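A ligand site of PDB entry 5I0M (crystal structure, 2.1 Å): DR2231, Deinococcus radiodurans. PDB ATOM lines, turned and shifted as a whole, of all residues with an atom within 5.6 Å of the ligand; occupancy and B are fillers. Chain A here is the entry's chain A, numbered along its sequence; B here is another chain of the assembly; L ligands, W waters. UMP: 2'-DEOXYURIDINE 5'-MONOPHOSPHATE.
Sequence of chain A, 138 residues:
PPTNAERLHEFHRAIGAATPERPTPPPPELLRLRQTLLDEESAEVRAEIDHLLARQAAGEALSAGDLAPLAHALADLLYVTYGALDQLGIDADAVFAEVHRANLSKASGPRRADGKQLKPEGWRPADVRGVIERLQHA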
ATOM      1  N   VAL A  99     -16.012  -6.911 -15.720  1.00  0.00           N
ATOM      2  CA  VAL A  99     -14.806  -6.091 -15.799  1.00  0.00           C
ATOM      3  C   VAL A  99     -14.853  -4.971 -14.768  1.00  0.00           C
ATOM      4  O   VAL A  99     -13.845  -4.654 -14.128  1.00  0.00           O
ATOM      5  CB  VAL A  99     -14.623  -5.558 -17.228  1.00  0.00           C
ATOM      6  CG1 VAL A  99     -13.537  -4.464 -17.263  1.00  0.00           C
ATOM      7  CG2 VAL A  99     -14.301  -6.718 -18.172  1.00  0.00           C
ATOM      8  N   ASN A 103     -12.343  -3.835 -11.629  1.00  0.00           N
ATOM      9  CA  ASN A 103     -11.612  -2.571 -11.631  1.00  0.00           C
ATOM     10  C   ASN A 103     -11.842  -1.793 -10.332  1.00  0.00           C
ATOM     11  O   ASN A 103     -10.915  -1.172  -9.824  1.00  0.00           O
ATOM     12  CB  ASN A 103     -12.015  -1.734 -12.854  1.00  0.00           C
ATOM     13  CG  ASN A 103     -11.395  -2.231 -14.131  1.00  0.00           C
ATOM     14  OD1 ASN A 103     -10.432  -3.003 -14.103  1.00  0.00           O
ATOM     15  ND2 ASN A 103     -11.919  -1.789 -15.259  1.00  0.00           N
ATOM     16  N   LYS A 106      -9.342  -2.470  -7.617  1.00  0.00           N
ATOM     17  CA  LYS A 106      -7.993  -1.936  -7.722  1.00  0.00           C
ATOM     18  C   LYS A 106      -7.767  -0.679  -6.880  1.00  0.00           C
ATOM     19  O   LYS A 106      -6.644  -0.165  -6.883  1.00  0.00           O
ATOM     20  CB  LYS A 106      -7.628  -1.609  -9.177  1.00  0.00           C
ATOM     21  CG  LYS A 106      -7.672  -2.774 -10.165  1.00  0.00           C
ATOM     22  CD  LYS A 106      -7.566  -2.302 -11.628  1.00  0.00           C
ATOM     23  CE  LYS A 106      -7.555  -3.488 -12.601  1.00  0.00           C
ATOM     24  NZ  LYS A 106      -7.466  -3.086 -14.061  1.00  0.00           N
ATOM     25  N   GLY A 115      -0.937   8.714 -14.163  1.00  0.00           N
ATOM     26  CA  GLY A 115      -2.223   8.641 -13.512  1.00  0.00           C
ATOM     27  C   GLY A 115      -2.954   7.327 -13.688  1.00  0.00           C
ATOM     28  O   GLY A 115      -4.037   7.175 -13.105  1.00  0.00           O
ATOM     29  N   LYS A 116      -2.417   6.383 -14.470  1.00  0.00           N
ATOM     30  CA  LYS A 116      -3.069   5.081 -14.587  1.00  0.00           C
ATOM     31  C   LYS A 116      -3.095   4.384 -13.235  1.00  0.00           C
ATOM     32  O   LYS A 116      -2.072   4.289 -12.555  1.00  0.00           O
ATOM     33  CB  LYS A 116      -2.367   4.189 -15.609  1.00  0.00           C
ATOM     34  CG  LYS A 116      -3.095   2.836 -15.816  1.00  0.00           C
ATOM     35  CD  LYS A 116      -2.360   1.922 -16.821  1.00  0.00           C
ATOM     36  CE  LYS A 116      -3.156   0.660 -17.086  1.00  0.00           C
ATOM     37  NZ  LYS A 116      -2.461  -0.299 -18.011  1.00  0.00           N
ATOM     38  N   GLN A 117      -4.287   3.935 -12.857  1.00  0.00           N
ATOM     39  CA  GLN A 117      -4.464   3.088 -11.686  1.00  0.00           C
ATOM     40  C   GLN A 117      -3.847   1.720 -11.957  1.00  0.00           C
ATOM     41  O   GLN A 117      -4.088   1.111 -12.994  1.00  0.00           O
ATOM     42  CB  GLN A 117      -5.952   2.937 -11.362  1.00  0.00           C
ATOM     43  CG  GLN A 117      -6.251   2.090 -10.126  1.00  0.00           C
ATOM     44  CD  GLN A 117      -5.639   2.704  -8.881  1.00  0.00           C
ATOM     45  OE1 GLN A 117      -5.892   3.855  -8.578  1.00  0.00           O
ATOM     46  NE2 GLN A 117      -4.811   1.937  -8.183  1.00  0.00           N
ATOM     47  N   LEU A 118      -3.033   1.234 -11.023  1.00  0.00           N
ATOM     48  CA  LEU A 118      -2.387  -0.065 -11.153  1.00  0.00           C
ATOM     49  C   LEU A 118      -2.968  -1.031 -10.108  1.00  0.00           C
ATOM     50  O   LEU A 118      -3.790  -0.665  -9.249  1.00  0.00           O
ATOM     51  CB  LEU A 118      -0.876   0.069 -11.016  1.00  0.00           C
ATOM     52  CG  LEU A 118      -0.258   1.028 -12.048  1.00  0.00           C
ATOM     53  CD1 LEU A 118       1.226   1.244 -11.730  1.00  0.00           C
ATOM     54  CD2 LEU A 118      -0.458   0.521 -13.494  1.00  0.00           C
ATOM     55  N   LYS A 119      -2.540  -2.277 -10.204  1.00  0.00           N
ATOM     56  CA  LYS A 119      -3.230  -3.298  -9.427  1.00  0.00           C
ATOM     57  C   LYS A 119      -2.573  -3.491  -8.072  1.00  0.00           C
ATOM     58  O   LYS A 119      -1.343  -3.525  -7.978  1.00  0.00           O
ATOM     59  CB  LYS A 119      -3.248  -4.614 -10.188  1.00  0.00           C
ATOM     60  CG  LYS A 119      -4.147  -4.586 -11.429  1.00  0.00           C
ATOM     61  CD  LYS A 119      -3.512  -5.316 -12.616  1.00  0.00           C
ATOM     62  CE  LYS A 119      -4.420  -5.249 -13.865  1.00  0.00           C
ATOM     63  NZ  LYS A 119      -3.823  -5.989 -15.014  1.00  0.00           N
ATOM     64  N   LEU B   8     -18.444   3.993 -14.760  1.00  0.00           N
ATOM     65  CA  LEU B   8     -17.171   4.716 -14.810  1.00  0.00           C
ATOM     66  C   LEU B   8     -17.123   5.812 -13.759  1.00  0.00           C
ATOM     67  O   LEU B   8     -16.081   6.027 -13.121  1.00  0.00           O
ATOM     68  CB  LEU B   8     -16.935   5.291 -16.215  1.00  0.00           C
ATOM     69  CG  LEU B   8     -15.958   4.446 -17.039  1.00  0.00           C
ATOM     70  CD1 LEU B   8     -14.607   4.410 -16.328  1.00  0.00           C
ATOM     71  CD2 LEU B   8     -16.451   3.030 -17.242  1.00  0.00           C
ATOM     72  N   PHE B  11     -16.145   4.236 -10.592  1.00  0.00           N
ATOM     73  CA  PHE B  11     -14.743   3.848 -10.584  1.00  0.00           C
ATOM     74  C   PHE B  11     -13.824   5.037 -10.313  1.00  0.00           C
ATOM     75  O   PHE B  11     -12.905   4.946  -9.494  1.00  0.00           O
ATOM     76  CB  PHE B  11     -14.374   3.202 -11.917  1.00  0.00           C
ATOM     77  CG  PHE B  11     -12.917   2.931 -12.079  1.00  0.00           C
ATOM     78  CD1 PHE B  11     -12.297   1.909 -11.350  1.00  0.00           C
ATOM     79  CD2 PHE B  11     -12.170   3.646 -12.985  1.00  0.00           C
ATOM     80  CE1 PHE B  11     -10.935   1.651 -11.514  1.00  0.00           C
ATOM     81  CE2 PHE B  11     -10.813   3.377 -13.170  1.00  0.00           C
ATOM     82  CZ  PHE B  11     -10.202   2.383 -12.429  1.00  0.00           C
ATOM     83  N   HIS B  12     -14.036   6.157 -11.001  1.00  0.00           N
ATOM     84  CA  HIS B  12     -13.119   7.278 -10.854  1.00  0.00           C
ATOM     85  C   HIS B  12     -13.216   7.906  -9.474  1.00  0.00           C
ATOM     86  O   HIS B  12     -12.211   8.372  -8.915  1.00  0.00           O
ATOM     87  CB  HIS B  12     -13.385   8.299 -11.958  1.00  0.00           C
ATOM     88  CG  HIS B  12     -12.818   7.884 -13.278  1.00  0.00           C
ATOM     89  ND1 HIS B  12     -13.355   8.280 -14.487  1.00  0.00           N
ATOM     90  CD2 HIS B  12     -11.762   7.079 -13.583  1.00  0.00           C
ATOM     91  CE1 HIS B  12     -12.653   7.745 -15.473  1.00  0.00           C
ATOM     92  NE2 HIS B  12     -11.676   7.019 -14.953  1.00  0.00           N
ATOM     93  N   ILE B  15     -11.156   5.771  -7.134  1.00  0.00           N
ATOM     94  CA  ILE B  15      -9.712   5.809  -7.255  1.00  0.00           C
ATOM     95  C   ILE B  15      -9.153   7.220  -7.086  1.00  0.00           C
ATOM     96  O   ILE B  15      -7.938   7.413  -7.233  1.00  0.00           O
ATOM     97  CB  ILE B  15      -9.210   5.212  -8.596  1.00  0.00           C
ATOM     98  CG1 ILE B  15      -9.594   6.106  -9.778  1.00  0.00           C
ATOM     99  CG2 ILE B  15      -9.722   3.800  -8.805  1.00  0.00           C
ATOM    100  CD1 ILE B  15      -8.892   5.683 -11.086  1.00  0.00           C
ATOM    101  N   LEU B  33      -3.041  10.956 -20.836  1.00  0.00           N
ATOM    102  CA  LEU B  33      -3.412   9.686 -20.216  1.00  0.00           C
ATOM    103  C   LEU B  33      -4.520   8.998 -21.011  1.00  0.00           C
ATOM    104  O   LEU B  33      -4.444   7.804 -21.274  1.00  0.00           O
ATOM    105  CB  LEU B  33      -3.846   9.888 -18.764  1.00  0.00           C
ATOM    106  CG  LEU B  33      -4.389   8.606 -18.097  1.00  0.00           C
ATOM    107  CD1 LEU B  33      -3.307   7.522 -17.985  1.00  0.00           C
ATOM    108  CD2 LEU B  33      -5.065   8.881 -16.709  1.00  0.00           C
ATOM    109  N   ARG B  34      -5.554   9.743 -21.399  1.00  0.00           N
ATOM    110  CA  ARG B  34      -6.661   9.088 -22.088  1.00  0.00           C
ATOM    111  C   ARG B  34      -6.185   8.494 -23.414  1.00  0.00           C
ATOM    112  O   ARG B  34      -6.634   7.414 -23.807  1.00  0.00           O
ATOM    113  CB  ARG B  34      -7.833  10.039 -22.330  1.00  0.00           C
ATOM    114  CG  ARG B  34      -8.493  10.647 -21.085  1.00  0.00           C
ATOM    115  CD  ARG B  34      -8.537   9.713 -19.885  1.00  0.00           C
ATOM    116  NE  ARG B  34      -9.235   8.459 -20.147  1.00  0.00           N
ATOM    117  CZ  ARG B  34      -9.599   7.613 -19.178  1.00  0.00           C
ATOM    118  NH1 ARG B  34      -9.361   7.935 -17.915  1.00  0.00           N
ATOM    119  NH2 ARG B  34     -10.197   6.466 -19.469  1.00  0.00           N
ATOM    120  N   LEU B  37      -4.248   5.164 -22.601  1.00  0.00           N
ATOM    121  CA  LEU B  37      -5.118   4.041 -22.254  1.00  0.00           C
ATOM    122  C   LEU B  37      -5.888   3.541 -23.475  1.00  0.00           C
ATOM    123  O   LEU B  37      -6.066   2.333 -23.646  1.00  0.00           O
ATOM    124  CB  LEU B  37      -6.078   4.459 -21.136  1.00  0.00           C
ATOM    125  CG  LEU B  37      -5.405   4.919 -19.822  1.00  0.00           C
ATOM    126  CD1 LEU B  37      -6.450   5.207 -18.755  1.00  0.00           C
ATOM    127  CD2 LEU B  37      -4.391   3.864 -19.329  1.00  0.00           C
ATOM    128  N   GLU B  40      -3.397   1.488 -25.411  1.00  0.00           N
ATOM    129  CA  GLU B  40      -3.151   0.212 -24.731  1.00  0.00           C
ATOM    130  C   GLU B  40      -4.259  -0.798 -25.033  1.00  0.00           C
ATOM    131  O   GLU B  40      -3.987  -1.927 -25.438  1.00  0.00           O
ATOM    132  CB  GLU B  40      -3.030   0.427 -23.213  1.00  0.00           C
ATOM    133  CG  GLU B  40      -1.803   1.257 -22.778  1.00  0.00           C
ATOM    134  CD  GLU B  40      -1.570   1.296 -21.253  1.00  0.00           C
ATOM    135  OE1 GLU B  40      -2.428   0.813 -20.472  1.00  0.00           O
ATOM    136  OE2 GLU B  40      -0.512   1.808 -20.841  1.00  0.00           O
ATOM    137  N   GLU B  41      -5.519  -0.403 -24.830  1.00  0.00           N
ATOM    138  CA  GLU B  41      -6.614  -1.359 -24.960  1.00  0.00           C
ATOM    139  C   GLU B  41      -6.939  -1.692 -26.407  1.00  0.00           C
ATOM    140  O   GLU B  41      -7.350  -2.820 -26.696  1.00  0.00           O
ATOM    141  CB  GLU B  41      -7.864  -0.851 -24.243  1.00  0.00           C
ATOM    142  CG  GLU B  41      -7.686  -0.613 -22.746  1.00  0.00           C
ATOM    143  CD  GLU B  41      -6.909  -1.721 -22.050  1.00  0.00           C
ATOM    144  OE1 GLU B  41      -7.114  -2.921 -22.379  1.00  0.00           O
ATOM    145  OE2 GLU B  41      -6.054  -1.405 -21.200  1.00  0.00           O
ATOM    146  N   ALA B  75     -14.421  -5.193 -23.831  1.00  0.00           N
ATOM    147  CA  ALA B  75     -14.990  -4.505 -22.672  1.00  0.00           C
ATOM    148  C   ALA B  75     -13.978  -3.548 -22.049  1.00  0.00           C
ATOM    149  O   ALA B  75     -14.362  -2.476 -21.581  1.00  0.00           O
ATOM    150  CB  ALA B  75     -15.472  -5.518 -21.628  1.00  0.00           C
ATOM    151  N   ASP B  76     -12.693  -3.915 -22.037  1.00  0.00           N
ATOM    152  CA  ASP B  76     -11.660  -3.007 -21.530  1.00  0.00           C
ATOM    153  C   ASP B  76     -11.610  -1.738 -22.369  1.00  0.00           C
ATOM    154  O   ASP B  76     -11.404  -0.640 -21.836  1.00  0.00           O
ATOM    155  CB  ASP B  76     -10.270  -3.657 -21.525  1.00  0.00           C
ATOM    156  CG  ASP B  76     -10.005  -4.528 -20.301  1.00  0.00           C
ATOM    157  OD1 ASP B  76     -10.758  -4.451 -19.295  1.00  0.00           O
ATOM    158  OD2 ASP B  76      -9.009  -5.293 -20.327  1.00  0.00           O
ATOM    159  N   TYR B  79     -14.242   0.412 -21.565  1.00  0.00           N
ATOM    160  CA  TYR B  79     -14.037   0.978 -20.246  1.00  0.00           C
ATOM    161  C   TYR B  79     -13.212   2.257 -20.317  1.00  0.00           C
ATOM    162  O   TYR B  79     -13.544   3.256 -19.678  1.00  0.00           O
ATOM    163  CB  TYR B  79     -13.396  -0.072 -19.323  1.00  0.00           C
ATOM    164  CG  TYR B  79     -13.748   0.114 -17.864  1.00  0.00           C
ATOM    165  CD1 TYR B  79     -13.019   0.990 -17.050  1.00  0.00           C
ATOM    166  CD2 TYR B  79     -14.821  -0.568 -17.297  1.00  0.00           C
ATOM    167  CE1 TYR B  79     -13.346   1.166 -15.697  1.00  0.00           C
ATOM    168  CE2 TYR B  79     -15.175  -0.395 -15.958  1.00  0.00           C
ATOM    169  CZ  TYR B  79     -14.429   0.471 -15.167  1.00  0.00           C
ATOM    170  OH  TYR B  79     -14.767   0.642 -13.846  1.00  0.00           O
ATOM    171  N   VAL B  80     -12.158   2.268 -21.140  1.00  0.00           N
ATOM    172  CA  VAL B  80     -11.338   3.473 -21.243  1.00  0.00           C
ATOM    173  C   VAL B  80     -11.948   4.522 -22.164  1.00  0.00           C
ATOM    174  O   VAL B  80     -11.585   5.701 -22.068  1.00  0.00           O
ATOM    175  CB  VAL B  80      -9.912   3.136 -21.718  1.00  0.00           C
ATOM    176  CG1 VAL B  80      -9.215   2.259 -20.697  1.00  0.00           C
ATOM    177  CG2 VAL B  80      -9.948   2.451 -23.095  1.00  0.00           C
HETATM  178  N1  UMP L   1      -8.531   1.087 -16.071  1.00  0.00           N
HETATM  179  C2  UMP L   1      -9.112   2.437 -16.178  1.00  0.00           C
HETATM  180  N3  UMP L   1      -8.318   3.599 -15.672  1.00  0.00           N
HETATM  181  C4  UMP L   1      -7.016   3.427 -15.085  1.00  0.00           C
HETATM  182  C5  UMP L   1      -6.452   2.061 -14.970  1.00  0.00           C
HETATM  183  C6  UMP L   1      -7.228   0.912 -15.460  1.00  0.00           C
HETATM  184  O2  UMP L   1     -10.184   2.594 -16.662  1.00  0.00           O
HETATM  185  O4  UMP L   1      -6.425   4.366 -14.688  1.00  0.00           O
HETATM  186  C1' UMP L   1      -9.306  -0.064 -16.537  1.00  0.00           C
HETATM  187  C2' UMP L   1      -9.400  -0.176 -18.098  1.00  0.00           C
HETATM  188  C3' UMP L   1      -9.427  -1.678 -18.320  1.00  0.00           C
HETATM  189  C4' UMP L   1      -8.561  -2.145 -17.401  1.00  0.00           C
HETATM  190  O3' UMP L   1     -10.788  -2.158 -18.005  1.00  0.00           O
HETATM  191  O4' UMP L   1      -8.686  -1.152 -16.142  1.00  0.00           O
HETATM  192  C5' UMP L   1      -7.149  -2.072 -17.891  1.00  0.00           C
HETATM  193  O5' UMP L   1      -6.257  -2.188 -16.802  1.00  0.00           O
HETATM  194  P   UMP L   1      -4.800  -2.950 -17.049  1.00  0.00           P
HETATM  195  OP1 UMP L   1      -3.878  -2.611 -15.892  1.00  0.00           O
HETATM  196  OP2 UMP L   1      -4.140  -2.492 -18.313  1.00  0.00           O
HETATM  197  OP3 UMP L   1      -5.016  -4.436 -17.131  1.00  0.00           O
HETATM  198  O   HOH W   1      -7.281  -5.161 -15.826  1.00  0.00           O
HETATM  199  O   HOH W   2      -7.233   7.038 -14.163  1.00  0.00           O
HETATM  200  O   HOH W   3      -1.529  -3.025 -14.956  1.00  0.00           O
HETATM  201  O   HOH W   4     -11.217   4.900 -17.403  1.00  0.00           O
HETATM  202  O   HOH W   5      -9.119   6.179 -15.578  1.00  0.00           O
HETATM  203  O   HOH W   6      -2.378  -4.448 -18.973  1.00  0.00           O
HETATM  204  O   HOH W   7      -5.041  -1.370 -13.760  1.00  0.00           O
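The side-chain carboxylate (OD1) of Asp 76 of chain B sits at hydrogen-bond distance from an oxygen (O3') of the ligand, 2.6 Å away. The side-chain amino group (NZ) of Lys 116 is in salt-bridge range of an oxygen (OP2) of the ligand, at 2.8 Å. An oxygen (O4) of the ligand lies within hydrogen-bond range of the backbone NH (N) of Gln 117, 2.8 Å away. OP3 of the ligand lies within salt-bridge range of NZ of Lys 119 (2.9 Å). The side-chain amide nitrogen (ND2) of Asn 103 is in hydrogen-bond range of an oxygen (O3') of the ligand, 3.0 Å away. An oxygen (O4') of the ligand lies within hydrogen-bond range of the side-chain amino group (NZ) of Lys 106, at 3.1 Å.
The side-chain amino group of Lys 116 is in salt-bridge range of the side-chain carboxylate of Glu 40 of chain B, at 2.7 Å. The side-chain amide nitrogen (NE2) of Gln 117 is in hydrogen-bond range of the backbone carbonyl oxygen (O) of Lys 106 (3.1 Å). NZ of Lys 106 is in hydrogen-bond range of OD1 of Asn 103. NH2 of Arg 34 of chain B is in hydrogen-bond range of O of Val 80 of chain B (3.0 Å).
Val 99 touches the ligand. CE2 of Phe 11 of chain B touches N3 of the ligand, at 3.5 Å. Leu 37 of chain B touches the ligand (CD1 to N3, 3.9 Å). OE2 of Glu 41 of chain B touches C5' of the ligand (3.5 Å). Tyr 79 of chain B touches the ligand (CD1 to O2, 3.3 Å). CG1 of Val 80 of chain B touches C2' of the ligand (3.6 Å). 12 residues have an atom within 4 Å of the ligand: Val 99, Asn 103, Lys 106, Lys 116, Gln 117, Lys 119, Phe 11 of chain B, Leu 37 of chain B, Glu 41 of chain B, Asp 76 of chain B, Tyr 79 of chain B and Val 80 of chain B. The nearest printed residue that does not touch the ligand is Gly 115 (4.01 Å).
Water W4 lies within hydrogen-bond range of O2 of the ligand (2.6 Å), NH2 of Arg 34 of chain B (2.8 Å) and NE2 of His 12 of chain B (3.3 Å). Water W5 lies within hydrogen-bond range of N3 of the ligand, NE2 of His 12 of chain B and NH1 of Arg 34 of chain B. Water W1 lies within hydrogen-bond range of an oxygen (OP3) of the ligand (2.7 Å) and the side-chain amino group of Lys 106 (2.7 Å). Water W7 lies within hydrogen-bond range of OP1 of the ligand (2.7 Å), O of Gln 117 (2.8 Å) and NZ of Lys 106 (3.0 Å). Water W2 bridges an oxygen (O4) of the ligand (2.8 Å) and the backbone carbonyl oxygen of Gly 115 (3.4 Å).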
